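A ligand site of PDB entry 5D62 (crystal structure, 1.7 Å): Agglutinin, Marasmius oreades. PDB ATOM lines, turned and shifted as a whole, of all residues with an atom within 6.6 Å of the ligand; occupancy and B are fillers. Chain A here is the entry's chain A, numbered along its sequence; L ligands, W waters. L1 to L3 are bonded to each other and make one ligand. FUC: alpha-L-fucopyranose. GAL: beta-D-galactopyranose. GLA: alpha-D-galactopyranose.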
ATOM      1  N   HIS A   9     -17.556  16.573  34.983  1.00  0.00           N
ATOM      2  CA  HIS A   9     -16.423  17.386  34.520  1.00  0.00           C
ATOM      3  C   HIS A   9     -15.222  16.528  34.959  1.00  0.00           C
ATOM      4  O   HIS A   9     -15.061  16.216  36.145  1.00  0.00           O
ATOM      5  CB  HIS A   9     -16.484  18.710  35.230  1.00  0.00           C
ATOM      6  CG  HIS A   9     -15.425  19.661  34.796  1.00  0.00           C
ATOM      7  ND1 HIS A   9     -14.281  19.920  35.532  1.00  0.00           N
ATOM      8  CD2 HIS A   9     -15.288  20.342  33.630  1.00  0.00           C
ATOM      9  CE1 HIS A   9     -13.545  20.782  34.874  1.00  0.00           C
ATOM     10  NE2 HIS A   9     -14.113  21.039  33.705  1.00  0.00           N
ATOM     11  N   ASP A  20     -11.508  17.805  27.317  1.00  0.00           N
ATOM     12  CA  ASP A  20     -12.136  18.877  26.564  1.00  0.00           C
ATOM     13  C   ASP A  20     -12.296  18.372  25.066  1.00  0.00           C
ATOM     14  O   ASP A  20     -11.355  17.950  24.431  1.00  0.00           O
ATOM     15  CB  ASP A  20     -11.254  20.099  26.627  1.00  0.00           C
ATOM     16  CG  ASP A  20     -11.848  21.382  25.944  1.00  0.00           C
ATOM     17  OD1 ASP A  20     -12.034  21.382  24.669  1.00  0.00           O
ATOM     18  OD2 ASP A  20     -12.086  22.440  26.622  1.00  0.00           O
ATOM     19  N   LEU A  21     -13.460  18.501  24.521  1.00  0.00           N
ATOM     20  CA  LEU A  21     -13.670  18.146  23.098  1.00  0.00           C
ATOM     21  C   LEU A  21     -13.384  19.449  22.357  1.00  0.00           C
ATOM     22  O   LEU A  21     -14.139  20.473  22.543  1.00  0.00           O
ATOM     23  CB  LEU A  21     -15.126  17.748  22.873  1.00  0.00           C
ATOM     24  CG  LEU A  21     -15.498  17.479  21.425  1.00  0.00           C
ATOM     25  CD1 LEU A  21     -14.705  16.333  20.827  1.00  0.00           C
ATOM     26  CD2 LEU A  21     -16.998  17.159  21.251  1.00  0.00           C
ATOM     27  N   LYS A  22     -12.358  19.454  21.551  1.00  0.00           N
ATOM     28  CA  LYS A  22     -11.816  20.722  20.987  1.00  0.00           C
ATOM     29  C   LYS A  22     -12.865  21.500  20.197  1.00  0.00           C
ATOM     30  O   LYS A  22     -13.507  20.990  19.270  1.00  0.00           O
ATOM     31  CB  LYS A  22     -10.500  20.479  20.185  1.00  0.00           C
ATOM     32  CG  LYS A  22      -9.610  21.640  20.274  1.00  0.00           C
ATOM     33  CD  LYS A  22      -8.351  21.395  19.402  1.00  0.00           C
ATOM     34  CE  LYS A  22      -7.496  22.669  19.547  1.00  0.00           C
ATOM     35  NZ  LYS A  22      -6.120  22.327  18.942  1.00  0.00           N
ATOM     36  N   ASP A  23     -13.005  22.777  20.577  1.00  0.00           N
ATOM     37  CA  ASP A  23     -14.031  23.691  20.064  1.00  0.00           C
ATOM     38  C   ASP A  23     -15.455  23.228  20.140  1.00  0.00           C
ATOM     39  O   ASP A  23     -16.310  23.767  19.451  1.00  0.00           O
ATOM     40  CB  ASP A  23     -13.697  24.053  18.601  1.00  0.00           C
ATOM     41  CG  ASP A  23     -14.168  25.456  18.204  1.00  0.00           C
ATOM     42  OD1 ASP A  23     -14.154  26.406  18.988  1.00  0.00           O
ATOM     43  OD2 ASP A  23     -14.582  25.619  17.038  1.00  0.00           O
ATOM     44  N   GLY A  24     -15.722  22.196  20.909  1.00  0.00           N
ATOM     45  CA  GLY A  24     -17.019  21.659  21.031  1.00  0.00           C
ATOM     46  C   GLY A  24     -17.511  21.068  19.724  1.00  0.00           C
ATOM     47  O   GLY A  24     -18.710  20.857  19.590  1.00  0.00           O
ATOM     48  N   VAL A  33      -8.804  16.684  24.255  1.00  0.00           N
ATOM     49  CA  VAL A  33      -7.550  17.273  24.649  1.00  0.00           C
ATOM     50  C   VAL A  33      -7.645  17.697  26.084  1.00  0.00           C
ATOM     51  O   VAL A  33      -8.767  17.937  26.628  1.00  0.00           O
ATOM     52  CB  VAL A  33      -7.121  18.550  23.782  1.00  0.00           C
ATOM     53  CG1 VAL A  33      -6.761  18.153  22.348  1.00  0.00           C
ATOM     54  CG2 VAL A  33      -8.168  19.628  23.787  1.00  0.00           C
ATOM     55  N   TRP A  35      -7.338  20.728  28.743  1.00  0.00           N
ATOM     56  CA  TRP A  35      -7.608  22.189  28.715  1.00  0.00           C
ATOM     57  C   TRP A  35      -7.915  22.700  30.113  1.00  0.00           C
ATOM     58  O   TRP A  35      -8.630  22.079  30.884  1.00  0.00           O
ATOM     59  CB  TRP A  35      -8.755  22.530  27.760  1.00  0.00           C
ATOM     60  CG  TRP A  35      -8.698  23.887  27.138  1.00  0.00           C
ATOM     61  CD1 TRP A  35      -8.980  25.078  27.720  1.00  0.00           C
ATOM     62  CD2 TRP A  35      -8.251  24.181  25.827  1.00  0.00           C
ATOM     63  NE1 TRP A  35      -8.762  26.130  26.835  1.00  0.00           N
ATOM     64  CE2 TRP A  35      -8.302  25.613  25.668  1.00  0.00           C
ATOM     65  CE3 TRP A  35      -7.804  23.380  24.760  1.00  0.00           C
ATOM     66  CZ2 TRP A  35      -7.911  26.263  24.480  1.00  0.00           C
ATOM     67  CZ3 TRP A  35      -7.394  24.032  23.583  1.00  0.00           C
ATOM     68  CH2 TRP A  35      -7.460  25.479  23.455  1.00  0.00           C
ATOM     69  N   GLN A  36      -7.476  23.913  30.427  1.00  0.00           N
ATOM     70  CA  GLN A  36      -7.809  24.539  31.685  1.00  0.00           C
ATOM     71  C   GLN A  36      -9.267  24.900  31.795  1.00  0.00           C
ATOM     72  O   GLN A  36      -9.969  24.970  30.809  1.00  0.00           O
ATOM     73  CB  GLN A  36      -6.931  25.779  31.950  1.00  0.00           C
ATOM     74  CG  GLN A  36      -7.236  26.969  31.079  1.00  0.00           C
ATOM     75  CD  GLN A  36      -6.290  28.143  31.339  1.00  0.00           C
ATOM     76  OE1 GLN A  36      -6.336  28.726  32.394  1.00  0.00           O
ATOM     77  NE2 GLN A  36      -5.426  28.463  30.398  1.00  0.00           N
ATOM     78  N   PHE A  37      -9.750  25.176  33.025  1.00  0.00           N
ATOM     79  CA  PHE A  37     -11.157  25.364  33.282  1.00  0.00           C
ATOM     80  C   PHE A  37     -11.358  26.415  34.348  1.00  0.00           C
ATOM     81  O   PHE A  37     -10.346  26.821  35.012  1.00  0.00           O
ATOM     82  CB  PHE A  37     -11.788  23.985  33.691  1.00  0.00           C
ATOM     83  CG  PHE A  37     -11.253  23.436  34.986  1.00  0.00           C
ATOM     84  CD1 PHE A  37     -10.195  22.578  34.978  1.00  0.00           C
ATOM     85  CD2 PHE A  37     -11.886  23.703  36.163  1.00  0.00           C
ATOM     86  CE1 PHE A  37      -9.709  22.020  36.162  1.00  0.00           C
ATOM     87  CE2 PHE A  37     -11.346  23.222  37.390  1.00  0.00           C
ATOM     88  CZ  PHE A  37     -10.271  22.376  37.333  1.00  0.00           C
ATOM     89  N   THR A  38     -12.599  26.864  34.468  1.00  0.00           N
ATOM     90  CA  THR A  38     -12.953  27.871  35.495  1.00  0.00           C
ATOM     91  C   THR A  38     -13.980  27.190  36.406  1.00  0.00           C
ATOM     92  O   THR A  38     -15.024  26.766  35.928  1.00  0.00           O
ATOM     93  CB  THR A  38     -13.518  29.162  34.831  1.00  0.00           C
ATOM     94  OG1 THR A  38     -12.557  29.618  33.838  1.00  0.00           O
ATOM     95  CG2 THR A  38     -13.795  30.211  35.860  1.00  0.00           C
ATOM     96  N   PRO A  39     -13.699  27.059  37.707  1.00  0.00           N
ATOM     97  CA  PRO A  39     -14.719  26.468  38.650  1.00  0.00           C
ATOM     98  C   PRO A  39     -15.956  27.305  38.784  1.00  0.00           C
ATOM     99  O   PRO A  39     -15.908  28.493  38.500  1.00  0.00           O
ATOM    100  CB  PRO A  39     -13.992  26.391  39.993  1.00  0.00           C
ATOM    101  CG  PRO A  39     -12.657  27.013  39.778  1.00  0.00           C
ATOM    102  CD  PRO A  39     -12.518  27.592  38.401  1.00  0.00           C
ATOM    103  N   THR A  41     -18.535  27.593  36.868  1.00  0.00           N
ATOM    104  CA  THR A  41     -19.039  28.089  35.602  1.00  0.00           C
ATOM    105  C   THR A  41     -19.535  26.840  34.843  1.00  0.00           C
ATOM    106  O   THR A  41     -19.168  25.713  35.212  1.00  0.00           O
ATOM    107  CB  THR A  41     -17.978  28.690  34.674  1.00  0.00           C
ATOM    108  OG1 THR A  41     -17.032  27.684  34.271  1.00  0.00           O
ATOM    109  CG2 THR A  41     -17.259  29.841  35.372  1.00  0.00           C
ATOM    110  N   ILE A  42     -20.292  27.063  33.785  1.00  0.00           N
ATOM    111  CA  ILE A  42     -20.501  26.034  32.752  1.00  0.00           C
ATOM    112  C   ILE A  42     -19.234  26.002  31.886  1.00  0.00           C
ATOM    113  O   ILE A  42     -18.940  27.013  31.155  1.00  0.00           O
ATOM    114  CB  ILE A  42     -21.744  26.317  31.896  1.00  0.00           C
ATOM    115  CG1 ILE A  42     -23.024  26.259  32.796  1.00  0.00           C
ATOM    116  CG2 ILE A  42     -21.761  25.361  30.703  1.00  0.00           C
ATOM    117  CD1 ILE A  42     -23.330  24.950  33.482  1.00  0.00           C
ATOM    118  N   ASN A  43     -18.502  24.870  31.916  1.00  0.00           N
ATOM    119  CA  ASN A  43     -17.356  24.654  30.972  1.00  0.00           C
ATOM    120  C   ASN A  43     -17.854  23.955  29.769  1.00  0.00           C
ATOM    121  O   ASN A  43     -18.046  22.699  29.784  1.00  0.00           O
ATOM    122  CB  ASN A  43     -16.220  23.894  31.697  1.00  0.00           C
ATOM    123  CG  ASN A  43     -15.589  24.764  32.785  1.00  0.00           C
ATOM    124  OD1 ASN A  43     -14.742  25.594  32.493  1.00  0.00           O
ATOM    125  ND2 ASN A  43     -15.957  24.540  34.080  1.00  0.00           N
ATOM    126  N   TRP A  44     -18.186  24.784  28.758  1.00  0.00           N
ATOM    127  CA  TRP A  44     -19.076  24.392  27.680  1.00  0.00           C
ATOM    128  C   TRP A  44     -18.601  23.175  26.902  1.00  0.00           C
ATOM    129  O   TRP A  44     -19.439  22.369  26.395  1.00  0.00           O
ATOM    130  CB  TRP A  44     -19.270  25.549  26.677  1.00  0.00           C
ATOM    131  CG  TRP A  44     -20.272  26.518  27.213  1.00  0.00           C
ATOM    132  CD1 TRP A  44     -20.001  27.706  27.898  1.00  0.00           C
ATOM    133  CD2 TRP A  44     -21.723  26.391  27.115  1.00  0.00           C
ATOM    134  NE1 TRP A  44     -21.226  28.285  28.272  1.00  0.00           N
ATOM    135  CE2 TRP A  44     -22.275  27.486  27.844  1.00  0.00           C
ATOM    136  CE3 TRP A  44     -22.579  25.408  26.559  1.00  0.00           C
ATOM    137  CZ2 TRP A  44     -23.647  27.701  27.951  1.00  0.00           C
ATOM    138  CZ3 TRP A  44     -23.928  25.581  26.699  1.00  0.00           C
ATOM    139  CH2 TRP A  44     -24.468  26.751  27.383  1.00  0.00           C
ATOM    140  N   HIS A  45     -17.289  23.012  26.752  1.00  0.00           N
ATOM    141  CA  HIS A  45     -16.806  21.822  25.972  1.00  0.00           C
ATOM    142  C   HIS A  45     -16.338  20.657  26.778  1.00  0.00           C
ATOM    143  O   HIS A  45     -15.781  19.681  26.251  1.00  0.00           O
ATOM    144  CB  HIS A  45     -15.742  22.268  24.980  1.00  0.00           C
ATOM    145  CG  HIS A  45     -16.154  23.451  24.147  1.00  0.00           C
ATOM    146  ND1 HIS A  45     -15.232  24.325  23.614  1.00  0.00           N
ATOM    147  CD2 HIS A  45     -17.350  23.803  23.648  1.00  0.00           C
ATOM    148  CE1 HIS A  45     -15.877  25.231  22.862  1.00  0.00           C
ATOM    149  NE2 HIS A  45     -17.147  24.911  22.839  1.00  0.00           N
ATOM    150  N   GLN A  46     -16.566  20.661  28.125  1.00  0.00           N
ATOM    151  CA  GLN A  46     -15.897  19.803  29.088  1.00  0.00           C
ATOM    152  C   GLN A  46     -16.882  18.984  29.927  1.00  0.00           C
ATOM    153  O   GLN A  46     -16.504  18.518  31.008  1.00  0.00           O
ATOM    154  CB  GLN A  46     -15.006  20.643  30.009  1.00  0.00           C
ATOM    155  CG  GLN A  46     -13.916  21.430  29.183  1.00  0.00           C
ATOM    156  CD  GLN A  46     -13.033  22.284  30.071  1.00  0.00           C
ATOM    157  OE1 GLN A  46     -13.261  22.376  31.310  1.00  0.00           O
ATOM    158  NE2 GLN A  46     -12.011  22.827  29.524  1.00  0.00           N
ATOM    159  N   PHE A  66     -22.402  19.145  25.068  1.00  0.00           N
ATOM    160  CA  PHE A  66     -22.518  20.133  24.027  1.00  0.00           C
ATOM    161  C   PHE A  66     -22.588  19.562  22.602  1.00  0.00           C
ATOM    162  O   PHE A  66     -23.533  19.939  21.868  1.00  0.00           O
ATOM    163  CB  PHE A  66     -21.351  21.115  24.086  1.00  0.00           C
ATOM    164  CG  PHE A  66     -21.440  22.240  23.096  1.00  0.00           C
ATOM    165  CD1 PHE A  66     -22.367  23.329  23.315  1.00  0.00           C
ATOM    166  CD2 PHE A  66     -20.670  22.290  21.957  1.00  0.00           C
ATOM    167  CE1 PHE A  66     -22.465  24.370  22.431  1.00  0.00           C
ATOM    168  CE2 PHE A  66     -20.733  23.409  21.068  1.00  0.00           C
ATOM    169  CZ  PHE A  66     -21.631  24.422  21.298  1.00  0.00           C
ATOM    170  N   ASP A 131      -2.878  24.003  27.237  1.00  0.00           N
ATOM    171  CA  ASP A 131      -4.222  23.991  26.646  1.00  0.00           C
ATOM    172  C   ASP A 131      -4.094  23.315  25.250  1.00  0.00           C
ATOM    173  O   ASP A 131      -3.293  23.748  24.351  1.00  0.00           O
ATOM    174  CB  ASP A 131      -4.809  25.418  26.519  1.00  0.00           C
ATOM    175  CG  ASP A 131      -5.200  25.995  27.861  1.00  0.00           C
ATOM    176  OD1 ASP A 131      -5.375  25.140  28.768  1.00  0.00           O
ATOM    177  OD2 ASP A 131      -5.315  27.245  27.949  1.00  0.00           O
HETATM  178  C1  FUC L   1     -14.712  29.321  26.445  1.00  0.00           C
HETATM  179  C2  FUC L   1     -14.668  30.852  26.487  1.00  0.00           C
HETATM  180  C3  FUC L   1     -15.336  31.399  25.208  1.00  0.00           C
HETATM  181  C4  FUC L   1     -16.755  30.800  24.941  1.00  0.00           C
HETATM  182  C5  FUC L   1     -16.550  29.251  24.830  1.00  0.00           C
HETATM  183  C6  FUC L   1     -17.877  28.488  24.645  1.00  0.00           C
HETATM  184  O2  FUC L   1     -13.298  31.214  26.671  1.00  0.00           O
HETATM  185  O3  FUC L   1     -15.404  32.831  25.403  1.00  0.00           O
HETATM  186  O4  FUC L   1     -17.661  31.191  26.027  1.00  0.00           O
HETATM  187  O5  FUC L   1     -15.977  28.782  26.070  1.00  0.00           O
HETATM  188  C1  GAL L   2     -13.066  27.536  23.686  1.00  0.00           C
HETATM  189  C2  GAL L   2     -13.583  27.501  25.146  1.00  0.00           C
HETATM  190  C3  GAL L   2     -12.573  26.921  26.108  1.00  0.00           C
HETATM  191  C4  GAL L   2     -12.084  25.543  25.673  1.00  0.00           C
HETATM  192  C5  GAL L   2     -11.726  25.630  24.134  1.00  0.00           C
HETATM  193  C6  GAL L   2     -11.294  24.303  23.562  1.00  0.00           C
HETATM  194  O1  GAL L   2     -14.206  27.830  22.901  1.00  0.00           O
HETATM  195  O2  GAL L   2     -13.739  28.930  25.433  1.00  0.00           O
HETATM  196  O3  GAL L   2     -13.141  26.928  27.442  1.00  0.00           O
HETATM  197  O4  GAL L   2     -13.182  24.643  25.857  1.00  0.00           O
HETATM  198  O5  GAL L   2     -12.796  26.188  23.301  1.00  0.00           O
HETATM  199  O6  GAL L   2     -12.373  23.394  23.291  1.00  0.00           O
HETATM  200  C1  GLA L   3     -12.158  26.488  28.457  1.00  0.00           C
HETATM  201  C2  GLA L   3     -12.925  26.693  29.791  1.00  0.00           C
HETATM  202  C3  GLA L   3     -12.973  28.150  30.271  1.00  0.00           C
HETATM  203  C4  GLA L   3     -11.585  28.827  30.205  1.00  0.00           C
HETATM  204  C5  GLA L   3     -11.131  28.643  28.736  1.00  0.00           C
HETATM  205  C6  GLA L   3      -9.801  29.256  28.404  1.00  0.00           C
HETATM  206  O2  GLA L   3     -14.260  26.130  29.821  1.00  0.00           O
HETATM  207  O3  GLA L   3     -13.483  28.201  31.639  1.00  0.00           O
HETATM  208  O4  GLA L   3     -10.676  28.148  31.110  1.00  0.00           O
HETATM  209  O5  GLA L   3     -10.943  27.252  28.494  1.00  0.00           O
HETATM  210  O6  GLA L   3      -9.335  29.017  27.033  1.00  0.00           O
HETATM  211  O   HOH W   1     -16.171  28.384  31.611  1.00  0.00           O
HETATM  212  O   HOH W   2     -15.165  24.482  27.779  1.00  0.00           O
HETATM  213  O   HOH W   3     -17.478  30.270  28.592  1.00  0.00           O
HETATM  214  O   HOH W   4     -10.977  30.502  25.271  1.00  0.00           O
HETATM  215  O   HOH W   5     -16.754  27.435  28.951  1.00  0.00           O
HETATM  216  O   HOH W   6      -6.492  29.191  25.914  1.00  0.00           O
HETATM  217  O   HOH W   7     -11.954  26.511  20.615  1.00  0.00           O
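A ring nitrogen (ND1) of His 45 lies within hydrogen-bond range of an oxygen (O6) of GAL L2 (3.0 Å).
The side-chain amide oxygen of Asn 43 is in hydrogen-bond range of an oxygen (O2) of GLA L3 (2.8 Å).
The indole nitrogen (NE1) of Trp 35 is in hydrogen-bond range of an oxygen (O6) of GLA L3.
N of Asp 23 lies within hydrogen-bond range of O6 of GAL L2 (2.9 Å).
The side-chain carboxylate (OD1) of Asp 20 lies within hydrogen-bond range of an oxygen (O6) of GAL L2, at 2.5 Å.
O6 of GAL L2 is in hydrogen-bond range of O of Leu 21 (3.5 Å).
N of Thr 38 sits at hydrogen-bond distance from O3 of GLA L3, at 3.3 Å.
An oxygen (O3) of GLA L3 sits at hydrogen-bond distance from the side-chain hydroxyl (OG1) of Thr 38 (2.8 Å).
An oxygen (O4) of GLA L3 is in hydrogen-bond range of the backbone carbonyl oxygen (O) of Gln 36, at 3.3 Å.
A ring nitrogen (ND1) of His 45 sits at hydrogen-bond distance from the backbone NH (N) of Gly 24 (3.5 Å).
O of Thr 38 is in hydrogen-bond range of OG1 of Thr 41, at 2.8 Å.
NE2 of Gln 46 sits at hydrogen-bond distance from O of Gln 36, at 3.2 Å.
The side-chain amide nitrogen (ND2) of Asn 43 sits at hydrogen-bond distance from the side-chain hydroxyl (OG1) of Thr 41.
NE2 of Gln 36 is in hydrogen-bond range of OD2 of Asp 131 (2.7 Å).
O of Val 33 is in hydrogen-bond range of N of Asp 20 (2.8 Å).
OD2 of Asp 20 is in hydrogen-bond range of NE2 of Gln 46, 2.9 Å away.
A ring nitrogen (NE2) of His 9 lies within hydrogen-bond range of the side-chain amide oxygen (OE1) of Gln 46, 2.9 Å away.
CA of Lys 22 touches O6 of GAL L2, at 3.6 Å.
CA of Phe 37 touches O4 of GLA L3, at 3.6 Å.
CB of Trp 44 touches C6 of FUC L1 (3.8 Å).
Gln 46 touches the ligand.
Hydrophobic or aromatic side chains within 4 Å of the ligand: Trp 35, Trp 44 and His 45.
Water W1 lies within hydrogen-bond range of an oxygen (O3) of GLA L3, the side-chain hydroxyl (OG1) of Thr 41, the backbone carbonyl oxygen (O) of Ile 42 and the side-chain amide oxygen (OD1) of Asn 43.
Water W2 lies within hydrogen-bond range of an oxygen (O4) of GAL L2 (2.8 Å), the backbone NH of His 45 (2.8 Å) and the backbone NH of Trp 44 (3.2 Å).
Water W7 bridges the side-chain carboxylate of Asp 23 and an oxygen (O5) of GAL L2.
Water W5 lies within hydrogen-bond range of an oxygen (O2) of GLA L3 (2.9 Å), the backbone NH (N) of Trp 44 (3.0 Å) and the backbone carbonyl oxygen (O) of Ile 42 (3.1 Å).
Water W6 bridges the side-chain carboxylate (OD2) of Asp 131 (3.1 Å) and an oxygen (O6) of GLA L3 (3.1 Å).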
